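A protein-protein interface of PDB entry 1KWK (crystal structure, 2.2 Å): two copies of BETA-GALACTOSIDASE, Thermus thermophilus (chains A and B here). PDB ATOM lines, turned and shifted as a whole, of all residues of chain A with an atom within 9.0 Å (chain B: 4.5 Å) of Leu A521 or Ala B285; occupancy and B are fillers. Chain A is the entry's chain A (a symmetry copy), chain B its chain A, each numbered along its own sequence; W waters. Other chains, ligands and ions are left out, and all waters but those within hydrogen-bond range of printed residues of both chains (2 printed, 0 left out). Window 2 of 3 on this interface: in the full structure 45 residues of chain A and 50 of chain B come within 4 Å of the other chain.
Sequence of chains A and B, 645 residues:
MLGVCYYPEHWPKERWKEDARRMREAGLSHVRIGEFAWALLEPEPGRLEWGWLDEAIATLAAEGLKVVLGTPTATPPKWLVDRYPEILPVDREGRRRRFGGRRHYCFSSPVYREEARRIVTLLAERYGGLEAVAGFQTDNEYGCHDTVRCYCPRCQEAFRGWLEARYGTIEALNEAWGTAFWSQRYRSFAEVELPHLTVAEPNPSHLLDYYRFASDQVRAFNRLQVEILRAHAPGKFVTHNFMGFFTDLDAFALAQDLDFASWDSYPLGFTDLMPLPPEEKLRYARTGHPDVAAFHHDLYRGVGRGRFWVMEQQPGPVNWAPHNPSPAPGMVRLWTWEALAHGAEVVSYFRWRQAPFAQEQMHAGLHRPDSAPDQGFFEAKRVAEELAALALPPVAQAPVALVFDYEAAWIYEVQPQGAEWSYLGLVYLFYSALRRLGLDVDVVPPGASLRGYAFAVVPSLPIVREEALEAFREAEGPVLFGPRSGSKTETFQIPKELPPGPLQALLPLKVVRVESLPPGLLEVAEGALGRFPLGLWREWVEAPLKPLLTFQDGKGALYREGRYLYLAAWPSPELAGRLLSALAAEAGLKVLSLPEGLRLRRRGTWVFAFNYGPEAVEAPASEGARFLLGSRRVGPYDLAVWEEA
Of chain B, only Leu B282 and Ala B285 come within 4 Å of Leu A521. Of chain A, only Pro A519 (3.6 Å), Gly A520 (3.7 Å) and Leu A521 (3.6 Å) come within 4 Å of Leu B282. Of the printed residues of chain B, Gly A520 touches Leu B282. Of the printed residues of chain A, Pro B325 touches Glu A515, Ser A516 and Leu A517. Glu A523 touches none of the printed residues of chain B. Phe A551 touches none of the printed residues of chain B. The nearest residue of chain B that does not touch Leu A521 is Arg B286 (4.2 Å). The nearest residue of chain A that does not touch Ala B285 is Pro A518 (4.1 Å).
No position is printed for both chains.
Glu A515 touches Pro B325. Arg B286 touches Leu A517 (NH2 to CD2, 3.5 Å). CD2 of Leu A517 touches CB of Pro B325 (3.8 Å). CD2 of Leu B282 touches O of Pro A519 (3.6 Å). Leu B282 touches Gly A520 (CD1 to O, 3.7 Å). Leu A521 touches Leu B282 (N to CD2, 3.6 Å). Leu A521 touches Ala B285.
Hydrophobic or aromatic side chains of chain B that line the printed part of chain A: Leu B282, Ala B285 and Pro B325. Among the printed residues, 9 pairs touch across the chains.
N of Leu A517 sits at hydrogen-bond distance from O of Leu A536. The backbone NH (N) of Glu A515 is in hydrogen-bond range of the backbone carbonyl oxygen (O) of Arg A538 (2.7 Å).
Water W1 bridges OE1 of Glu A523 (2.6 Å) and NH1 of Arg B286 (2.9 Å). Water W2 lies within hydrogen-bond range of the guanidinium group of Arg A538, the guanidinium group of Arg B286 and the side-chain carboxylate of Glu A523.
OE1 of Glu A515 is in salt-bridge range of NE of Arg B286. The backbone carbonyl oxygen (O) of Ser A516 sits close to the backbone nitrogen (N) of Pro B325 (3.2 Å).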
ATOM      1  N   GLU A 420      23.716  -8.593   7.131  1.00  0.00           N
ATOM      2  CA  GLU A 420      23.112  -7.362   7.629  1.00  0.00           C
ATOM      3  C   GLU A 420      21.691  -7.557   8.160  1.00  0.00           C
ATOM      4  O   GLU A 420      21.055  -6.593   8.576  1.00  0.00           O
ATOM      5  CB  GLU A 420      23.103  -6.273   6.549  1.00  0.00           C
ATOM      6  CG  GLU A 420      24.482  -5.797   6.097  1.00  0.00           C
ATOM      7  CD  GLU A 420      25.235  -6.849   5.297  1.00  0.00           C
ATOM      8  OE1 GLU A 420      24.636  -7.437   4.368  1.00  0.00           O
ATOM      9  OE2 GLU A 420      26.427  -7.078   5.594  1.00  0.00           O
ATOM     10  N   GLU A 515      16.605 -14.124  -0.776  1.00  0.00           N
ATOM     11  CA  GLU A 515      17.953 -13.683  -1.121  1.00  0.00           C
ATOM     12  C   GLU A 515      18.476 -12.728  -0.068  1.00  0.00           C
ATOM     13  O   GLU A 515      17.726 -11.909   0.458  1.00  0.00           O
ATOM     14  CB  GLU A 515      17.986 -12.885  -2.432  1.00  0.00           C
ATOM     15  CG  GLU A 515      17.350 -13.488  -3.658  1.00  0.00           C
ATOM     16  CD  GLU A 515      17.621 -12.627  -4.888  1.00  0.00           C
ATOM     17  OE1 GLU A 515      18.780 -12.608  -5.375  1.00  0.00           O
ATOM     18  OE2 GLU A 515      16.677 -11.958  -5.355  1.00  0.00           O
ATOM     19  N   SER A 516      19.766 -12.830   0.231  1.00  0.00           N
ATOM     20  CA  SER A 516      20.404 -11.890   1.140  1.00  0.00           C
ATOM     21  C   SER A 516      21.393 -11.258   0.157  1.00  0.00           C
ATOM     22  O   SER A 516      22.118 -11.964  -0.558  1.00  0.00           O
ATOM     23  CB  SER A 516      21.094 -12.593   2.324  1.00  0.00           C
ATOM     24  OG  SER A 516      22.106 -13.498   1.927  1.00  0.00           O
ATOM     25  N   LEU A 517      21.371  -9.931   0.088  1.00  0.00           N
ATOM     26  CA  LEU A 517      22.196  -9.189  -0.854  1.00  0.00           C
ATOM     27  C   LEU A 517      23.272  -8.327  -0.197  1.00  0.00           C
ATOM     28  O   LEU A 517      23.091  -7.825   0.919  1.00  0.00           O
ATOM     29  CB  LEU A 517      21.277  -8.304  -1.713  1.00  0.00           C
ATOM     30  CG  LEU A 517      20.122  -9.022  -2.430  1.00  0.00           C
ATOM     31  CD1 LEU A 517      19.148  -8.011  -3.017  1.00  0.00           C
ATOM     32  CD2 LEU A 517      20.686  -9.904  -3.529  1.00  0.00           C
ATOM     33  N   PRO A 518      24.412  -8.143  -0.885  1.00  0.00           N
ATOM     34  CA  PRO A 518      25.510  -7.334  -0.353  1.00  0.00           C
ATOM     35  C   PRO A 518      25.134  -5.856  -0.266  1.00  0.00           C
ATOM     36  O   PRO A 518      24.380  -5.353  -1.095  1.00  0.00           O
ATOM     37  CB  PRO A 518      26.637  -7.585  -1.355  1.00  0.00           C
ATOM     38  CG  PRO A 518      25.901  -7.793  -2.634  1.00  0.00           C
ATOM     39  CD  PRO A 518      24.771  -8.703  -2.202  1.00  0.00           C
ATOM     40  N   PRO A 519      25.649  -5.142   0.749  1.00  0.00           N
ATOM     41  CA  PRO A 519      25.320  -3.717   0.874  1.00  0.00           C
ATOM     42  C   PRO A 519      25.655  -2.934  -0.398  1.00  0.00           C
ATOM     43  O   PRO A 519      26.687  -3.165  -1.035  1.00  0.00           O
ATOM     44  CB  PRO A 519      26.143  -3.272   2.090  1.00  0.00           C
ATOM     45  CG  PRO A 519      27.294  -4.236   2.105  1.00  0.00           C
ATOM     46  CD  PRO A 519      26.624  -5.552   1.774  1.00  0.00           C
ATOM     47  N   GLY A 520      24.772  -2.014  -0.768  1.00  0.00           N
ATOM     48  CA  GLY A 520      24.992  -1.227  -1.968  1.00  0.00           C
ATOM     49  C   GLY A 520      24.192  -1.761  -3.141  1.00  0.00           C
ATOM     50  O   GLY A 520      23.925  -1.031  -4.093  1.00  0.00           O
ATOM     51  N   LEU A 521      23.802  -3.035  -3.082  1.00  0.00           N
ATOM     52  CA  LEU A 521      23.024  -3.625  -4.163  1.00  0.00           C
ATOM     53  C   LEU A 521      21.564  -3.274  -3.928  1.00  0.00           C
ATOM     54  O   LEU A 521      20.912  -3.841  -3.052  1.00  0.00           O
ATOM     55  CB  LEU A 521      23.205  -5.150  -4.205  1.00  0.00           C
ATOM     56  CG  LEU A 521      23.031  -5.776  -5.606  1.00  0.00           C
ATOM     57  CD1 LEU A 521      23.385  -7.251  -5.567  1.00  0.00           C
ATOM     58  CD2 LEU A 521      21.608  -5.584  -6.101  1.00  0.00           C
ATOM     59  N   LEU A 522      21.059  -2.332  -4.718  1.00  0.00           N
ATOM     60  CA  LEU A 522      19.683  -1.875  -4.588  1.00  0.00           C
ATOM     61  C   LEU A 522      18.905  -1.989  -5.894  1.00  0.00           C
ATOM     62  O   LEU A 522      19.465  -1.864  -6.975  1.00  0.00           O
ATOM     63  CB  LEU A 522      19.674  -0.411  -4.132  1.00  0.00           C
ATOM     64  CG  LEU A 522      20.472  -0.073  -2.872  1.00  0.00           C
ATOM     65  CD1 LEU A 522      20.592   1.435  -2.729  1.00  0.00           C
ATOM     66  CD2 LEU A 522      19.790  -0.681  -1.661  1.00  0.00           C
ATOM     67  N   GLU A 523      17.606  -2.239  -5.778  1.00  0.00           N
ATOM     68  CA  GLU A 523      16.728  -2.330  -6.939  1.00  0.00           C
ATOM     69  C   GLU A 523      15.431  -1.641  -6.550  1.00  0.00           C
ATOM     70  O   GLU A 523      14.900  -1.860  -5.456  1.00  0.00           O
ATOM     71  CB  GLU A 523      16.446  -3.784  -7.331  1.00  0.00           C
ATOM     72  CG  GLU A 523      15.676  -3.909  -8.658  1.00  0.00           C
ATOM     73  CD  GLU A 523      15.406  -5.350  -9.075  1.00  0.00           C
ATOM     74  OE1 GLU A 523      16.323  -6.196  -8.960  1.00  0.00           O
ATOM     75  OE2 GLU A 523      14.280  -5.637  -9.533  1.00  0.00           O
ATOM     76  N   VAL A 524      14.925  -0.804  -7.448  1.00  0.00           N
ATOM     77  CA  VAL A 524      13.696  -0.067  -7.195  1.00  0.00           C
ATOM     78  C   VAL A 524      12.447  -0.929  -7.194  1.00  0.00           C
ATOM     79  O   VAL A 524      12.223  -1.731  -8.104  1.00  0.00           O
ATOM     80  CB  VAL A 524      13.491   1.061  -8.239  1.00  0.00           C
ATOM     81  CG1 VAL A 524      12.094   1.675  -8.081  1.00  0.00           C
ATOM     82  CG2 VAL A 524      14.555   2.138  -8.064  1.00  0.00           C
ATOM     83  N   PRO A 533      14.221   2.291  -3.579  1.00  0.00           N
ATOM     84  CA  PRO A 533      15.402   1.461  -3.829  1.00  0.00           C
ATOM     85  C   PRO A 533      15.499   0.576  -2.584  1.00  0.00           C
ATOM     86  O   PRO A 533      15.550   1.088  -1.466  1.00  0.00           O
ATOM     87  CB  PRO A 533      16.542   2.480  -3.891  1.00  0.00           C
ATOM     88  CG  PRO A 533      15.848   3.762  -4.295  1.00  0.00           C
ATOM     89  CD  PRO A 533      14.588   3.713  -3.481  1.00  0.00           C
ATOM     90  N   LEU A 534      15.498  -0.739  -2.774  1.00  0.00           N
ATOM     91  CA  LEU A 534      15.566  -1.667  -1.645  1.00  0.00           C
ATOM     92  C   LEU A 534      16.693  -2.681  -1.835  1.00  0.00           C
ATOM     93  O   LEU A 534      17.110  -2.956  -2.959  1.00  0.00           O
ATOM     94  CB  LEU A 534      14.223  -2.408  -1.486  1.00  0.00           C
ATOM     95  CG  LEU A 534      12.943  -1.583  -1.264  1.00  0.00           C
ATOM     96  CD1 LEU A 534      11.707  -2.498  -1.236  1.00  0.00           C
ATOM     97  CD2 LEU A 534      13.050  -0.815   0.042  1.00  0.00           C
ATOM     98  N   GLY A 535      17.182  -3.231  -0.729  1.00  0.00           N
ATOM     99  CA  GLY A 535      18.247  -4.213  -0.801  1.00  0.00           C
ATOM    100  C   GLY A 535      18.282  -5.078   0.443  1.00  0.00           C
ATOM    101  O   GLY A 535      17.258  -5.264   1.104  1.00  0.00           O
ATOM    102  N   LEU A 536      19.459  -5.621   0.737  1.00  0.00           N
ATOM    103  CA  LEU A 536      19.692  -6.454   1.914  1.00  0.00           C
ATOM    104  C   LEU A 536      18.965  -7.795   1.927  1.00  0.00           C
ATOM    105  O   LEU A 536      19.601  -8.846   2.046  1.00  0.00           O
ATOM    106  CB  LEU A 536      19.343  -5.666   3.183  1.00  0.00           C
ATOM    107  CG  LEU A 536      19.917  -6.167   4.514  1.00  0.00           C
ATOM    108  CD1 LEU A 536      19.920  -5.010   5.514  1.00  0.00           C
ATOM    109  CD2 LEU A 536      19.113  -7.361   5.042  1.00  0.00           C
ATOM    110  N   TRP A 537      17.641  -7.763   1.814  1.00  0.00           N
ATOM    111  CA  TRP A 537      16.838  -8.982   1.834  1.00  0.00           C
ATOM    112  C   TRP A 537      15.686  -8.895   0.837  1.00  0.00           C
ATOM    113  O   TRP A 537      14.981  -7.890   0.764  1.00  0.00           O
ATOM    114  CB  TRP A 537      16.296  -9.231   3.245  1.00  0.00           C
ATOM    115  CG  TRP A 537      15.582 -10.535   3.399  1.00  0.00           C
ATOM    116  CD1 TRP A 537      14.267 -10.785   3.143  1.00  0.00           C
ATOM    117  CD2 TRP A 537      16.152 -11.777   3.823  1.00  0.00           C
ATOM    118  NE1 TRP A 537      13.980 -12.108   3.381  1.00  0.00           N
ATOM    119  CE2 TRP A 537      15.121 -12.740   3.800  1.00  0.00           C
ATOM    120  CE3 TRP A 537      17.437 -12.169   4.218  1.00  0.00           C
ATOM    121  CZ2 TRP A 537      15.334 -14.075   4.160  1.00  0.00           C
ATOM    122  CZ3 TRP A 537      17.649 -13.495   4.576  1.00  0.00           C
ATOM    123  CH2 TRP A 537      16.602 -14.433   4.544  1.00  0.00           C
ATOM    124  N   ARG A 538      15.495  -9.963   0.075  1.00  0.00           N
ATOM    125  CA  ARG A 538      14.447  -9.989  -0.932  1.00  0.00           C
ATOM    126  C   ARG A 538      13.857 -11.388  -1.057  1.00  0.00           C
ATOM    127  O   ARG A 538      14.583 -12.376  -1.014  1.00  0.00           O
ATOM    128  CB  ARG A 538      15.031  -9.533  -2.266  1.00  0.00           C
ATOM    129  CG  ARG A 538      14.054  -9.545  -3.391  1.00  0.00           C
ATOM    130  CD  ARG A 538      14.672  -9.000  -4.650  1.00  0.00           C
ATOM    131  NE  ARG A 538      13.766  -9.216  -5.767  1.00  0.00           N
ATOM    132  CZ  ARG A 538      13.906  -8.662  -6.960  1.00  0.00           C
ATOM    133  NH1 ARG A 538      14.926  -7.850  -7.203  1.00  0.00           N
ATOM    134  NH2 ARG A 538      13.011  -8.912  -7.904  1.00  0.00           N
ATOM    135  N   PHE A 551       9.299  -5.001  -8.254  1.00  0.00           N
ATOM    136  CA  PHE A 551      10.687  -4.755  -8.614  1.00  0.00           C
ATOM    137  C   PHE A 551      10.799  -4.701 -10.131  1.00  0.00           C
ATOM    138  O   PHE A 551       9.839  -5.000 -10.843  1.00  0.00           O
ATOM    139  CB  PHE A 551      11.599  -5.854  -8.076  1.00  0.00           C
ATOM    140  CG  PHE A 551      11.931  -5.705  -6.620  1.00  0.00           C
ATOM    141  CD1 PHE A 551      11.355  -6.541  -5.671  1.00  0.00           C
ATOM    142  CD2 PHE A 551      12.847  -4.740  -6.203  1.00  0.00           C
ATOM    143  CE1 PHE A 551      11.690  -6.422  -4.321  1.00  0.00           C
ATOM    144  CE2 PHE A 551      13.187  -4.611  -4.857  1.00  0.00           C
ATOM    145  CZ  PHE A 551      12.608  -5.455  -3.914  1.00  0.00           C
ATOM    146  N   LEU B 268      28.498 -18.010  -6.562  1.00  0.00           N
ATOM    147  CA  LEU B 268      27.989 -16.911  -5.752  1.00  0.00           C
ATOM    148  C   LEU B 268      28.655 -16.831  -4.389  1.00  0.00           C
ATOM    149  O   LEU B 268      28.994 -15.746  -3.926  1.00  0.00           O
ATOM    150  CB  LEU B 268      26.475 -17.025  -5.582  1.00  0.00           C
ATOM    151  CG  LEU B 268      25.663 -17.118  -6.874  1.00  0.00           C
ATOM    152  CD1 LEU B 268      24.222 -16.769  -6.551  1.00  0.00           C
ATOM    153  CD2 LEU B 268      26.213 -16.170  -7.940  1.00  0.00           C
ATOM    154  N   LYS B 281      31.628  -6.351  -7.118  1.00  0.00           N
ATOM    155  CA  LYS B 281      30.933  -7.127  -6.095  1.00  0.00           C
ATOM    156  C   LYS B 281      29.419  -7.023  -6.284  1.00  0.00           C
ATOM    157  O   LYS B 281      28.680  -7.959  -5.989  1.00  0.00           O
ATOM    158  CB  LYS B 281      31.314  -6.629  -4.695  1.00  0.00           C
ATOM    159  CG  LYS B 281      30.664  -5.302  -4.341  1.00  0.00           C
ATOM    160  CD  LYS B 281      31.261  -4.663  -3.103  1.00  0.00           C
ATOM    161  CE  LYS B 281      30.687  -3.264  -2.903  1.00  0.00           C
ATOM    162  NZ  LYS B 281      31.424  -2.517  -1.846  1.00  0.00           N
ATOM    163  N   LEU B 282      28.962  -5.879  -6.781  1.00  0.00           N
ATOM    164  CA  LEU B 282      27.537  -5.674  -7.000  1.00  0.00           C
ATOM    165  C   LEU B 282      27.119  -6.242  -8.354  1.00  0.00           C
ATOM    166  O   LEU B 282      26.073  -6.883  -8.481  1.00  0.00           O
ATOM    167  CB  LEU B 282      27.202  -4.177  -6.946  1.00  0.00           C
ATOM    168  CG  LEU B 282      27.589  -3.426  -5.670  1.00  0.00           C
ATOM    169  CD1 LEU B 282      27.136  -1.973  -5.778  1.00  0.00           C
ATOM    170  CD2 LEU B 282      26.953  -4.091  -4.457  1.00  0.00           C
ATOM    171  N   ARG B 283      27.952  -6.009  -9.360  1.00  0.00           N
ATOM    172  CA  ARG B 283      27.666  -6.472 -10.710  1.00  0.00           C
ATOM    173  C   ARG B 283      27.605  -7.992 -10.844  1.00  0.00           C
ATOM    174  O   ARG B 283      26.795  -8.525 -11.606  1.00  0.00           O
ATOM    175  CB  ARG B 283      28.716  -5.915 -11.677  1.00  0.00           C
ATOM    176  CG  ARG B 283      28.549  -6.387 -13.099  1.00  0.00           C
ATOM    177  CD  ARG B 283      29.588  -5.766 -14.017  1.00  0.00           C
ATOM    178  NE  ARG B 283      29.523  -6.343 -15.358  1.00  0.00           N
ATOM    179  CZ  ARG B 283      30.259  -5.940 -16.391  1.00  0.00           C
ATOM    180  NH1 ARG B 283      31.128  -4.943 -16.250  1.00  0.00           N
ATOM    181  NH2 ARG B 283      30.125  -6.536 -17.570  1.00  0.00           N
ATOM    182  N   TYR B 284      28.453  -8.685 -10.095  1.00  0.00           N
ATOM    183  CA  TYR B 284      28.523 -10.141 -10.162  1.00  0.00           C
ATOM    184  C   TYR B 284      27.959 -10.871  -8.949  1.00  0.00           C
ATOM    185  O   TYR B 284      28.268 -12.042  -8.727  1.00  0.00           O
ATOM    186  CB  TYR B 284      29.978 -10.564 -10.377  1.00  0.00           C
ATOM    187  CG  TYR B 284      30.597  -9.988 -11.637  1.00  0.00           C
ATOM    188  CD1 TYR B 284      29.995 -10.178 -12.884  1.00  0.00           C
ATOM    189  CD2 TYR B 284      31.783  -9.260 -11.581  1.00  0.00           C
ATOM    190  CE1 TYR B 284      30.563  -9.653 -14.044  1.00  0.00           C
ATOM    191  CE2 TYR B 284      32.361  -8.731 -12.738  1.00  0.00           C
ATOM    192  CZ  TYR B 284      31.749  -8.929 -13.959  1.00  0.00           C
ATOM    193  OH  TYR B 284      32.313  -8.394 -15.093  1.00  0.00           O
ATOM    194  N   ALA B 285      27.134 -10.184  -8.167  1.00  0.00           N
ATOM    195  CA  ALA B 285      26.538 -10.780  -6.975  1.00  0.00           C
ATOM    196  C   ALA B 285      25.676 -11.990  -7.308  1.00  0.00           C
ATOM    197  O   ALA B 285      25.675 -12.976  -6.573  1.00  0.00           O
ATOM    198  CB  ALA B 285      25.699  -9.739  -6.234  1.00  0.00           C
ATOM    199  N   ARG B 286      24.942 -11.911  -8.415  1.00  0.00           N
ATOM    200  CA  ARG B 286      24.060 -12.999  -8.828  1.00  0.00           C
ATOM    201  C   ARG B 286      24.597 -13.857  -9.967  1.00  0.00           C
ATOM    202  O   ARG B 286      23.877 -14.702 -10.501  1.00  0.00           O
ATOM    203  CB  ARG B 286      22.694 -12.441  -9.238  1.00  0.00           C
ATOM    204  CG  ARG B 286      21.920 -11.738  -8.118  1.00  0.00           C
ATOM    205  CD  ARG B 286      20.452 -11.603  -8.510  1.00  0.00           C
ATOM    206  NE  ARG B 286      19.609 -11.048  -7.454  1.00  0.00           N
ATOM    207  CZ  ARG B 286      19.374  -9.753  -7.278  1.00  0.00           C
ATOM    208  NH1 ARG B 286      19.922  -8.851  -8.083  1.00  0.00           N
ATOM    209  NH2 ARG B 286      18.560  -9.360  -6.310  1.00  0.00           N
ATOM    210  N   THR B 287      25.854 -13.654 -10.343  1.00  0.00           N
ATOM    211  CA  THR B 287      26.430 -14.427 -11.436  1.00  0.00           C
ATOM    212  C   THR B 287      27.745 -15.073 -11.045  1.00  0.00           C
ATOM    213  O   THR B 287      28.109 -16.124 -11.570  1.00  0.00           O
ATOM    214  CB  THR B 287      26.723 -13.532 -12.666  1.00  0.00           C
ATOM    215  OG1 THR B 287      27.774 -12.611 -12.335  1.00  0.00           O
ATOM    216  CG2 THR B 287      25.475 -12.749 -13.082  1.00  0.00           C
ATOM    217  N   PRO B 325      22.841 -14.373  -2.563  1.00  0.00           N
ATOM    218  CA  PRO B 325      21.860 -13.975  -3.569  1.00  0.00           C
ATOM    219  C   PRO B 325      21.421 -15.190  -4.361  1.00  0.00           C
ATOM    220  O   PRO B 325      22.018 -16.267  -4.264  1.00  0.00           O
ATOM    221  CB  PRO B 325      22.636 -12.993  -4.454  1.00  0.00           C
ATOM    222  CG  PRO B 325      23.815 -12.583  -3.622  1.00  0.00           C
ATOM    223  CD  PRO B 325      24.174 -13.852  -2.908  1.00  0.00           C
HETATM  224  O   HOH W   1      18.905  -6.210  -8.664  1.00  0.00           O
HETATM  225  O   HOH W   2      17.324  -6.649  -6.063  1.00  0.00           O
